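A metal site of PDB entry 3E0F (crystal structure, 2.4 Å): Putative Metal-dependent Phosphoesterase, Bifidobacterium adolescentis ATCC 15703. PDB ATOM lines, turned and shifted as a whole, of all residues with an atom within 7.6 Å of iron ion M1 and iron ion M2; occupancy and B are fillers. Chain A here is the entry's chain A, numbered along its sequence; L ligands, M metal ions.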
ATOM      1  N   HIS A  18     -13.769 -26.840 -22.268  1.00  0.00           N
ATOM      2  CA  HIS A  18     -13.690 -25.716 -23.203  1.00  0.00           C
ATOM      3  C   HIS A  18     -12.262 -25.582 -23.836  1.00  0.00           C
ATOM      4  O   HIS A  18     -11.421 -24.787 -23.426  1.00  0.00           O
ATOM      5  CB  HIS A  18     -14.113 -24.451 -22.427  1.00  0.00           C
ATOM      6  CG  HIS A  18     -14.395 -23.268 -23.283  1.00  0.00           C
ATOM      7  ND1 HIS A  18     -15.016 -22.135 -22.790  1.00  0.00           N
ATOM      8  CD2 HIS A  18     -14.141 -23.020 -24.594  1.00  0.00           C
ATOM      9  CE1 HIS A  18     -15.120 -21.250 -23.766  1.00  0.00           C
ATOM     10  NE2 HIS A  18     -14.592 -21.747 -24.859  1.00  0.00           N
ATOM     11  N   CYS A  19     -12.014 -26.389 -24.869  1.00  0.00           N
ATOM     12  CA  CYS A  19     -10.693 -26.480 -25.497  1.00  0.00           C
ATOM     13  C   CYS A  19     -10.822 -26.447 -27.001  1.00  0.00           C
ATOM     14  O   CYS A  19     -11.680 -27.094 -27.555  1.00  0.00           O
ATOM     15  CB  CYS A  19     -10.024 -27.791 -25.101  1.00  0.00           C
ATOM     16  SG  CYS A  19     -10.030 -28.190 -23.358  1.00  0.00           S
ATOM     17  N   HIS A  20      -9.968 -25.675 -27.652  1.00  0.00           N
ATOM     18  CA  HIS A  20      -9.947 -25.516 -29.087  1.00  0.00           C
ATOM     19  C   HIS A  20      -8.737 -26.220 -29.730  1.00  0.00           C
ATOM     20  O   HIS A  20      -7.651 -26.296 -29.131  1.00  0.00           O
ATOM     21  CB  HIS A  20      -9.912 -24.034 -29.392  1.00  0.00           C
ATOM     22  CG  HIS A  20     -11.110 -23.305 -28.877  1.00  0.00           C
ATOM     23  ND1 HIS A  20     -12.246 -23.136 -29.626  1.00  0.00           N
ATOM     24  CD2 HIS A  20     -11.372 -22.746 -27.673  1.00  0.00           C
ATOM     25  CE1 HIS A  20     -13.153 -22.492 -28.916  1.00  0.00           C
ATOM     26  NE2 HIS A  20     -12.639 -22.234 -27.732  1.00  0.00           N
ATOM     27  N   ASP A  25      -9.513 -22.459 -34.029  1.00  0.00           N
ATOM     28  CA  ASP A  25      -8.416 -21.509 -33.826  1.00  0.00           C
ATOM     29  C   ASP A  25      -7.413 -21.890 -32.755  1.00  0.00           C
ATOM     30  O   ASP A  25      -6.640 -21.052 -32.314  1.00  0.00           O
ATOM     31  CB  ASP A  25      -8.964 -20.121 -33.513  1.00  0.00           C
ATOM     32  CG  ASP A  25      -9.900 -20.110 -32.297  1.00  0.00           C
ATOM     33  OD1 ASP A  25     -10.185 -21.186 -31.737  1.00  0.00           O
ATOM     34  OD2 ASP A  25     -10.368 -19.011 -31.929  1.00  0.00           O
ATOM     35  N   ALA A  48     -14.285 -28.188 -28.142  1.00  0.00           N
ATOM     36  CA  ALA A  48     -15.269 -27.071 -28.192  1.00  0.00           C
ATOM     37  C   ALA A  48     -14.922 -26.071 -29.305  1.00  0.00           C
ATOM     38  O   ALA A  48     -14.848 -24.854 -29.075  1.00  0.00           O
ATOM     39  CB  ALA A  48     -15.376 -26.368 -26.817  1.00  0.00           C
ATOM     40  N   ASP A  49     -14.737 -26.591 -30.506  1.00  0.00           N
ATOM     41  CA  ASP A  49     -14.286 -25.771 -31.621  1.00  0.00           C
ATOM     42  C   ASP A  49     -15.426 -24.913 -32.109  1.00  0.00           C
ATOM     43  O   ASP A  49     -16.563 -25.299 -32.003  1.00  0.00           O
ATOM     44  CB  ASP A  49     -13.694 -26.628 -32.775  1.00  0.00           C
ATOM     45  CG  ASP A  49     -12.279 -27.160 -32.461  1.00  0.00           C
ATOM     46  OD1 ASP A  49     -11.422 -26.373 -32.010  1.00  0.00           O
ATOM     47  OD2 ASP A  49     -12.030 -28.369 -32.674  1.00  0.00           O
ATOM     48  N   HIS A  50     -15.078 -23.737 -32.638  1.00  0.00           N
ATOM     49  CA  HIS A  50     -16.044 -22.822 -33.204  1.00  0.00           C
ATOM     50  C   HIS A  50     -16.811 -23.391 -34.359  1.00  0.00           C
ATOM     51  O   HIS A  50     -16.213 -23.772 -35.365  1.00  0.00           O
ATOM     52  CB  HIS A  50     -15.389 -21.536 -33.686  1.00  0.00           C
ATOM     53  CG  HIS A  50     -14.692 -20.787 -32.620  1.00  0.00           C
ATOM     54  ND1 HIS A  50     -15.371 -20.090 -31.644  1.00  0.00           N
ATOM     55  CD2 HIS A  50     -13.378 -20.652 -32.336  1.00  0.00           C
ATOM     56  CE1 HIS A  50     -14.502 -19.518 -30.830  1.00  0.00           C
ATOM     57  NE2 HIS A  50     -13.286 -19.843 -31.226  1.00  0.00           N
ATOM     58  N   GLU A  75     -18.331 -24.586 -29.728  1.00  0.00           N
ATOM     59  CA  GLU A  75     -18.618 -23.235 -29.292  1.00  0.00           C
ATOM     60  C   GLU A  75     -19.284 -22.485 -30.455  1.00  0.00           C
ATOM     61  O   GLU A  75     -18.767 -22.417 -31.558  1.00  0.00           O
ATOM     62  CB  GLU A  75     -17.340 -22.503 -28.858  1.00  0.00           C
ATOM     63  CG  GLU A  75     -17.622 -21.103 -28.349  1.00  0.00           C
ATOM     64  CD  GLU A  75     -16.459 -20.427 -27.676  1.00  0.00           C
ATOM     65  OE1 GLU A  75     -15.346 -20.964 -27.692  1.00  0.00           O
ATOM     66  OE2 GLU A  75     -16.660 -19.305 -27.131  1.00  0.00           O
ATOM     67  N   ILE A  76     -20.470 -21.934 -30.184  1.00  0.00           N
ATOM     68  CA  ILE A  76     -21.289 -21.287 -31.190  1.00  0.00           C
ATOM     69  C   ILE A  76     -21.324 -19.813 -30.855  1.00  0.00           C
ATOM     70  O   ILE A  76     -21.656 -19.428 -29.733  1.00  0.00           O
ATOM     71  CB  ILE A  76     -22.737 -21.855 -31.211  1.00  0.00           C
ATOM     72  CG1 ILE A  76     -22.700 -23.376 -31.255  1.00  0.00           C
ATOM     73  CG2 ILE A  76     -23.499 -21.307 -32.395  1.00  0.00           C
ATOM     74  CD1 ILE A  76     -24.060 -24.065 -30.982  1.00  0.00           C
ATOM     75  N   THR A  77     -20.953 -18.951 -31.803  1.00  0.00           N
ATOM     76  CA  THR A  77     -21.128 -17.512 -31.589  1.00  0.00           C
ATOM     77  C   THR A  77     -22.572 -17.146 -31.882  1.00  0.00           C
ATOM     78  O   THR A  77     -23.158 -17.595 -32.857  1.00  0.00           O
ATOM     79  CB  THR A  77     -20.195 -16.622 -32.448  1.00  0.00           C
ATOM     80  OG1 THR A  77     -18.857 -17.146 -32.408  1.00  0.00           O
ATOM     81  CG2 THR A  77     -20.234 -15.155 -31.929  1.00  0.00           C
ATOM     82  N   VAL A  85     -22.446 -13.208 -27.689  1.00  0.00           N
ATOM     83  CA  VAL A  85     -22.568 -14.290 -26.707  1.00  0.00           C
ATOM     84  C   VAL A  85     -21.987 -15.592 -27.279  1.00  0.00           C
ATOM     85  O   VAL A  85     -22.276 -15.969 -28.411  1.00  0.00           O
ATOM     86  CB  VAL A  85     -24.068 -14.584 -26.317  1.00  0.00           C
ATOM     87  CG1 VAL A  85     -24.137 -15.577 -25.178  1.00  0.00           C
ATOM     88  CG2 VAL A  85     -24.782 -13.317 -25.944  1.00  0.00           C
ATOM     89  N   HIS A  86     -21.151 -16.279 -26.507  1.00  0.00           N
ATOM     90  CA  HIS A  86     -20.633 -17.550 -26.987  1.00  0.00           C
ATOM     91  C   HIS A  86     -21.292 -18.674 -26.193  1.00  0.00           C
ATOM     92  O   HIS A  86     -21.455 -18.573 -24.969  1.00  0.00           O
ATOM     93  CB  HIS A  86     -19.123 -17.619 -26.846  1.00  0.00           C
ATOM     94  CG  HIS A  86     -18.375 -16.628 -27.678  1.00  0.00           C
ATOM     95  ND1 HIS A  86     -17.006 -16.702 -27.876  1.00  0.00           N
ATOM     96  CD2 HIS A  86     -18.791 -15.563 -28.400  1.00  0.00           C
ATOM     97  CE1 HIS A  86     -16.622 -15.707 -28.650  1.00  0.00           C
ATOM     98  NE2 HIS A  86     -17.687 -15.003 -28.984  1.00  0.00           N
ATOM     99  N   MET A  87     -21.656 -19.739 -26.877  1.00  0.00           N
ATOM    100  CA  MET A  87     -22.381 -20.818 -26.271  1.00  0.00           C
ATOM    101  C   MET A  87     -21.672 -22.123 -26.501  1.00  0.00           C
ATOM    102  O   MET A  87     -21.279 -22.448 -27.614  1.00  0.00           O
ATOM    103  CB  MET A  87     -23.769 -20.886 -26.863  1.00  0.00           C
ATOM    104  CG  MET A  87     -24.364 -19.499 -27.035  1.00  0.00           C
ATOM    105  SD  MET A  87     -26.150 -19.437 -26.403  1.00  0.00           S
ATOM    106  CE  MET A  87     -25.776 -19.442 -24.516  1.00  0.00           C
ATOM    107  N   LEU A  88     -21.494 -22.874 -25.425  1.00  0.00           N
ATOM    108  CA  LEU A  88     -20.944 -24.199 -25.521  1.00  0.00           C
ATOM    109  C   LEU A  88     -22.120 -25.157 -25.707  1.00  0.00           C
ATOM    110  O   LEU A  88     -23.091 -25.128 -24.951  1.00  0.00           O
ATOM    111  CB  LEU A  88     -20.134 -24.522 -24.268  1.00  0.00           C
ATOM    112  CG  LEU A  88     -19.017 -23.534 -23.967  1.00  0.00           C
ATOM    113  CD1 LEU A  88     -18.405 -23.786 -22.577  1.00  0.00           C
ATOM    114  CD2 LEU A  88     -17.962 -23.609 -25.054  1.00  0.00           C
ATOM    115  N   ALA A 202     -21.120 -19.390 -22.390  1.00  0.00           N
ATOM    116  CA  ALA A 202     -19.679 -19.340 -22.162  1.00  0.00           C
ATOM    117  C   ALA A 202     -19.271 -17.936 -21.724  1.00  0.00           C
ATOM    118  O   ALA A 202     -19.748 -16.957 -22.292  1.00  0.00           O
ATOM    119  CB  ALA A 202     -18.909 -19.729 -23.481  1.00  0.00           C
ATOM    120  N   HIS A 203     -18.355 -17.873 -20.737  1.00  0.00           N
ATOM    121  CA  HIS A 203     -17.777 -16.621 -20.192  1.00  0.00           C
ATOM    122  C   HIS A 203     -18.700 -15.384 -20.220  1.00  0.00           C
ATOM    123  O   HIS A 203     -18.306 -14.333 -20.728  1.00  0.00           O
ATOM    124  CB  HIS A 203     -16.440 -16.307 -20.889  1.00  0.00           C
ATOM    125  CG  HIS A 203     -16.517 -16.263 -22.380  1.00  0.00           C
ATOM    126  ND1 HIS A 203     -17.128 -15.241 -23.072  1.00  0.00           N
ATOM    127  CD2 HIS A 203     -16.017 -17.112 -23.319  1.00  0.00           C
ATOM    128  CE1 HIS A 203     -17.019 -15.460 -24.378  1.00  0.00           C
ATOM    129  NE2 HIS A 203     -16.356 -16.594 -24.543  1.00  0.00           N
ATOM    130  N   ASP A 206     -17.478 -11.885 -19.000  1.00  0.00           N
ATOM    131  CA  ASP A 206     -16.254 -11.347 -19.621  1.00  0.00           C
ATOM    132  C   ASP A 206     -16.521 -10.047 -20.464  1.00  0.00           C
ATOM    133  O   ASP A 206     -17.124 -10.115 -21.544  1.00  0.00           O
ATOM    134  CB  ASP A 206     -15.604 -12.458 -20.472  1.00  0.00           C
ATOM    135  CG  ASP A 206     -14.216 -12.114 -20.977  1.00  0.00           C
ATOM    136  OD1 ASP A 206     -13.745 -10.967 -20.825  1.00  0.00           O
ATOM    137  OD2 ASP A 206     -13.565 -13.025 -21.542  1.00  0.00           O
ATOM    138  N   GLU A 231     -21.021 -20.998 -17.760  1.00  0.00           N
ATOM    139  CA  GLU A 231     -19.610 -21.197 -17.484  1.00  0.00           C
ATOM    140  C   GLU A 231     -19.206 -20.101 -16.502  1.00  0.00           C
ATOM    141  O   GLU A 231     -19.167 -18.939 -16.842  1.00  0.00           O
ATOM    142  CB  GLU A 231     -18.804 -21.142 -18.776  1.00  0.00           C
ATOM    143  CG  GLU A 231     -17.322 -21.465 -18.652  1.00  0.00           C
ATOM    144  CD  GLU A 231     -16.599 -21.434 -20.011  1.00  0.00           C
ATOM    145  OE1 GLU A 231     -16.721 -20.423 -20.714  1.00  0.00           O
ATOM    146  OE2 GLU A 231     -15.914 -22.420 -20.370  1.00  0.00           O
ATOM    147  N   HIS A 234     -13.898 -19.390 -15.407  1.00  0.00           N
ATOM    148  CA  HIS A 234     -13.227 -19.024 -16.631  1.00  0.00           C
ATOM    149  C   HIS A 234     -12.441 -17.756 -16.324  1.00  0.00           C
ATOM    150  O   HIS A 234     -12.910 -16.878 -15.592  1.00  0.00           O
ATOM    151  CB  HIS A 234     -14.266 -18.762 -17.708  1.00  0.00           C
ATOM    152  CG  HIS A 234     -13.688 -18.451 -19.053  1.00  0.00           C
ATOM    153  ND1 HIS A 234     -13.126 -17.234 -19.348  1.00  0.00           N
ATOM    154  CD2 HIS A 234     -13.642 -19.172 -20.180  1.00  0.00           C
ATOM    155  CE1 HIS A 234     -12.721 -17.238 -20.590  1.00  0.00           C
ATOM    156  NE2 HIS A 234     -13.038 -18.390 -21.132  1.00  0.00           N
ATOM    157  N   SER A 260     -10.789 -24.011 -19.640  1.00  0.00           N
ATOM    158  CA  SER A 260      -9.593 -23.210 -19.814  1.00  0.00           C
ATOM    159  C   SER A 260      -9.719 -22.257 -20.976  1.00  0.00           C
ATOM    160  O   SER A 260      -9.109 -21.211 -20.960  1.00  0.00           O
ATOM    161  CB  SER A 260      -8.403 -24.095 -20.046  1.00  0.00           C
ATOM    162  OG  SER A 260      -8.542 -24.801 -21.255  1.00  0.00           O
ATOM    163  N   ASP A 261     -10.516 -22.601 -21.995  1.00  0.00           N
ATOM    164  CA  ASP A 261     -10.554 -21.848 -23.243  1.00  0.00           C
ATOM    165  C   ASP A 261      -9.192 -21.918 -23.958  1.00  0.00           C
ATOM    166  O   ASP A 261      -8.748 -20.997 -24.627  1.00  0.00           O
ATOM    167  CB  ASP A 261     -10.983 -20.414 -22.991  1.00  0.00           C
ATOM    168  CG  ASP A 261     -11.837 -19.903 -24.047  1.00  0.00           C
ATOM    169  OD1 ASP A 261     -11.747 -20.443 -25.146  1.00  0.00           O
ATOM    170  OD2 ASP A 261     -12.615 -18.984 -23.789  1.00  0.00           O
ATOM    171  N   TRP A 262      -8.552 -23.053 -23.764  1.00  0.00           N
ATOM    172  CA  TRP A 262      -7.256 -23.332 -24.290  1.00  0.00           C
ATOM    173  C   TRP A 262      -7.300 -23.256 -25.783  1.00  0.00           C
ATOM    174  O   TRP A 262      -8.179 -23.844 -26.418  1.00  0.00           O
ATOM    175  CB  TRP A 262      -6.915 -24.752 -23.917  1.00  0.00           C
ATOM    176  CG  TRP A 262      -5.582 -25.262 -24.297  1.00  0.00           C
ATOM    177  CD1 TRP A 262      -4.371 -24.882 -23.776  1.00  0.00           C
ATOM    178  CD2 TRP A 262      -5.316 -26.349 -25.191  1.00  0.00           C
ATOM    179  NE1 TRP A 262      -3.376 -25.651 -24.326  1.00  0.00           N
ATOM    180  CE2 TRP A 262      -3.931 -26.566 -25.181  1.00  0.00           C
ATOM    181  CE3 TRP A 262      -6.124 -27.158 -25.994  1.00  0.00           C
ATOM    182  CZ2 TRP A 262      -3.335 -27.538 -25.949  1.00  0.00           C
ATOM    183  CZ3 TRP A 262      -5.538 -28.119 -26.746  1.00  0.00           C
ATOM    184  CH2 TRP A 262      -4.158 -28.306 -26.735  1.00  0.00           C
ATOM    185  N   HIS A 263      -6.313 -22.553 -26.334  1.00  0.00           N
ATOM    186  CA  HIS A 263      -6.094 -22.531 -27.749  1.00  0.00           C
ATOM    187  C   HIS A 263      -4.681 -22.980 -28.026  1.00  0.00           C
ATOM    188  O   HIS A 263      -4.123 -22.634 -29.053  1.00  0.00           O
ATOM    189  CB  HIS A 263      -6.293 -21.116 -28.288  1.00  0.00           C
ATOM    190  CG  HIS A 263      -7.716 -20.679 -28.307  1.00  0.00           C
ATOM    191  ND1 HIS A 263      -8.460 -20.502 -27.167  1.00  0.00           N
ATOM    192  CD2 HIS A 263      -8.524 -20.364 -29.335  1.00  0.00           C
ATOM    193  CE1 HIS A 263      -9.661 -20.099 -27.491  1.00  0.00           C
ATOM    194  NE2 HIS A 263      -9.728 -20.007 -28.798  1.00  0.00           N
ATOM    195  N   LYS A 267      -3.016 -18.687 -27.229  1.00  0.00           N
ATOM    196  CA  LYS A 267      -3.469 -17.937 -26.056  1.00  0.00           C
ATOM    197  C   LYS A 267      -2.611 -18.319 -24.854  1.00  0.00           C
ATOM    198  O   LYS A 267      -2.053 -19.416 -24.816  1.00  0.00           O
ATOM    199  CB  LYS A 267      -4.928 -18.286 -25.694  1.00  0.00           C
ATOM    200  CG  LYS A 267      -6.010 -17.811 -26.666  1.00  0.00           C
ATOM    201  CD  LYS A 267      -6.883 -16.734 -26.097  1.00  0.00           C
ATOM    202  CE  LYS A 267      -8.336 -16.810 -26.620  1.00  0.00           C
ATOM    203  NZ  LYS A 267      -9.245 -17.680 -25.754  1.00  0.00           N
ATOM    204  N   ASN A 269      -3.904 -19.020 -21.978  1.00  0.00           N
ATOM    205  CA  ASN A 269      -4.735 -19.938 -21.196  1.00  0.00           C
ATOM    206  C   ASN A 269      -4.183 -21.331 -21.196  1.00  0.00           C
ATOM    207  O   ASN A 269      -3.886 -21.874 -22.258  1.00  0.00           O
ATOM    208  CB  ASN A 269      -6.180 -20.042 -21.749  1.00  0.00           C
ATOM    209  CG  ASN A 269      -6.847 -18.706 -21.932  1.00  0.00           C
ATOM    210  OD1 ASN A 269      -6.187 -17.713 -22.237  1.00  0.00           O
ATOM    211  ND2 ASN A 269      -8.165 -18.678 -21.787  1.00  0.00           N
HETATM  212  P1  LIG L   1     -12.768 -17.801 -27.985  1.00  0.00           P
HETATM  213  O1  LIG L   1     -12.007 -17.291 -26.766  1.00  0.00           O
HETATM  214  O2  LIG L   1     -14.227 -17.372 -28.066  1.00  0.00           O
HETATM  215  O3  LIG L   1     -12.007 -17.337 -29.209  1.00  0.00           O
HETATM  216  O4  LIG L   1     -12.878 -19.310 -27.871  1.00  0.00           O
HETATM  217 FE    FE M   1     -13.680 -20.583 -26.502  1.00  0.00          FE
HETATM  218 FE    FE M   2     -15.554 -17.677 -26.595  1.00  0.00          FE
HETATM  219 ZN    ZN M   3     -11.507 -19.359 -30.143  1.00  0.00          ZN
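A ring nitrogen (ND1) of His 263 sits at hydrogen-bond distance from the backbone carbonyl oxygen of Asp 261, at 2.6 Å.
The backbone carbonyl oxygen (O) of His 18 lies within hydrogen-bond range of the backbone NH (N) of Trp 262.
A ring nitrogen (NE2) of His 234 is in hydrogen-bond range of the side-chain carboxylate (OD2) of Asp 261 (2.8 Å).
A ring nitrogen (ND1) of His 20 lies close to the backbone carbonyl oxygen (O) of Ala 48 (3.2 Å).
ND1 of His 18 is in hydrogen-bond range of OE2 of Glu 231.
OD1 of Asp 261 sits close to NZ of Lys 267, 3.8 Å away.
The backbone NH of His 203 sits at hydrogen-bond distance from the side-chain carboxylate of Glu 231 (3.0 Å).
The backbone NH of His 20 is in hydrogen-bond range of the backbone carbonyl oxygen of Trp 262, at 2.8 Å.
Four residues have an atom within 4 Å of iron ion M1: His 18, His 20, Glu 75 and Asp 261.
Along chain A the residues within 4 Å of iron ion M1 span positions 18 to 261.
Of the 25 residues printed, 3 come within 4 Å of iron ion M2.
The nearest printed residue that does not touch iron ion M2 is Asp 261 (4.3 Å).
An oxygen (O4) of the ligand is bound to iron ion M1, at 2.0 Å.
OE1 of Glu 75 is bound to iron ion M1.
Iron ion M1 is bound by a ring nitrogen (NE2) of His 18 (2.2 Å).
NE2 of His 20 binds iron ion M1 (2.3 Å).
Iron ion M1 is bound by OD1 of Asp 261 (2.4 Å).
Iron ion M2 is bound by O2 of the ligand (2.0 Å), OE2 of Glu 75 (2.0 Å), ND1 of His 86 (2.2 Å) and NE2 of His 203 (2.5 Å).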
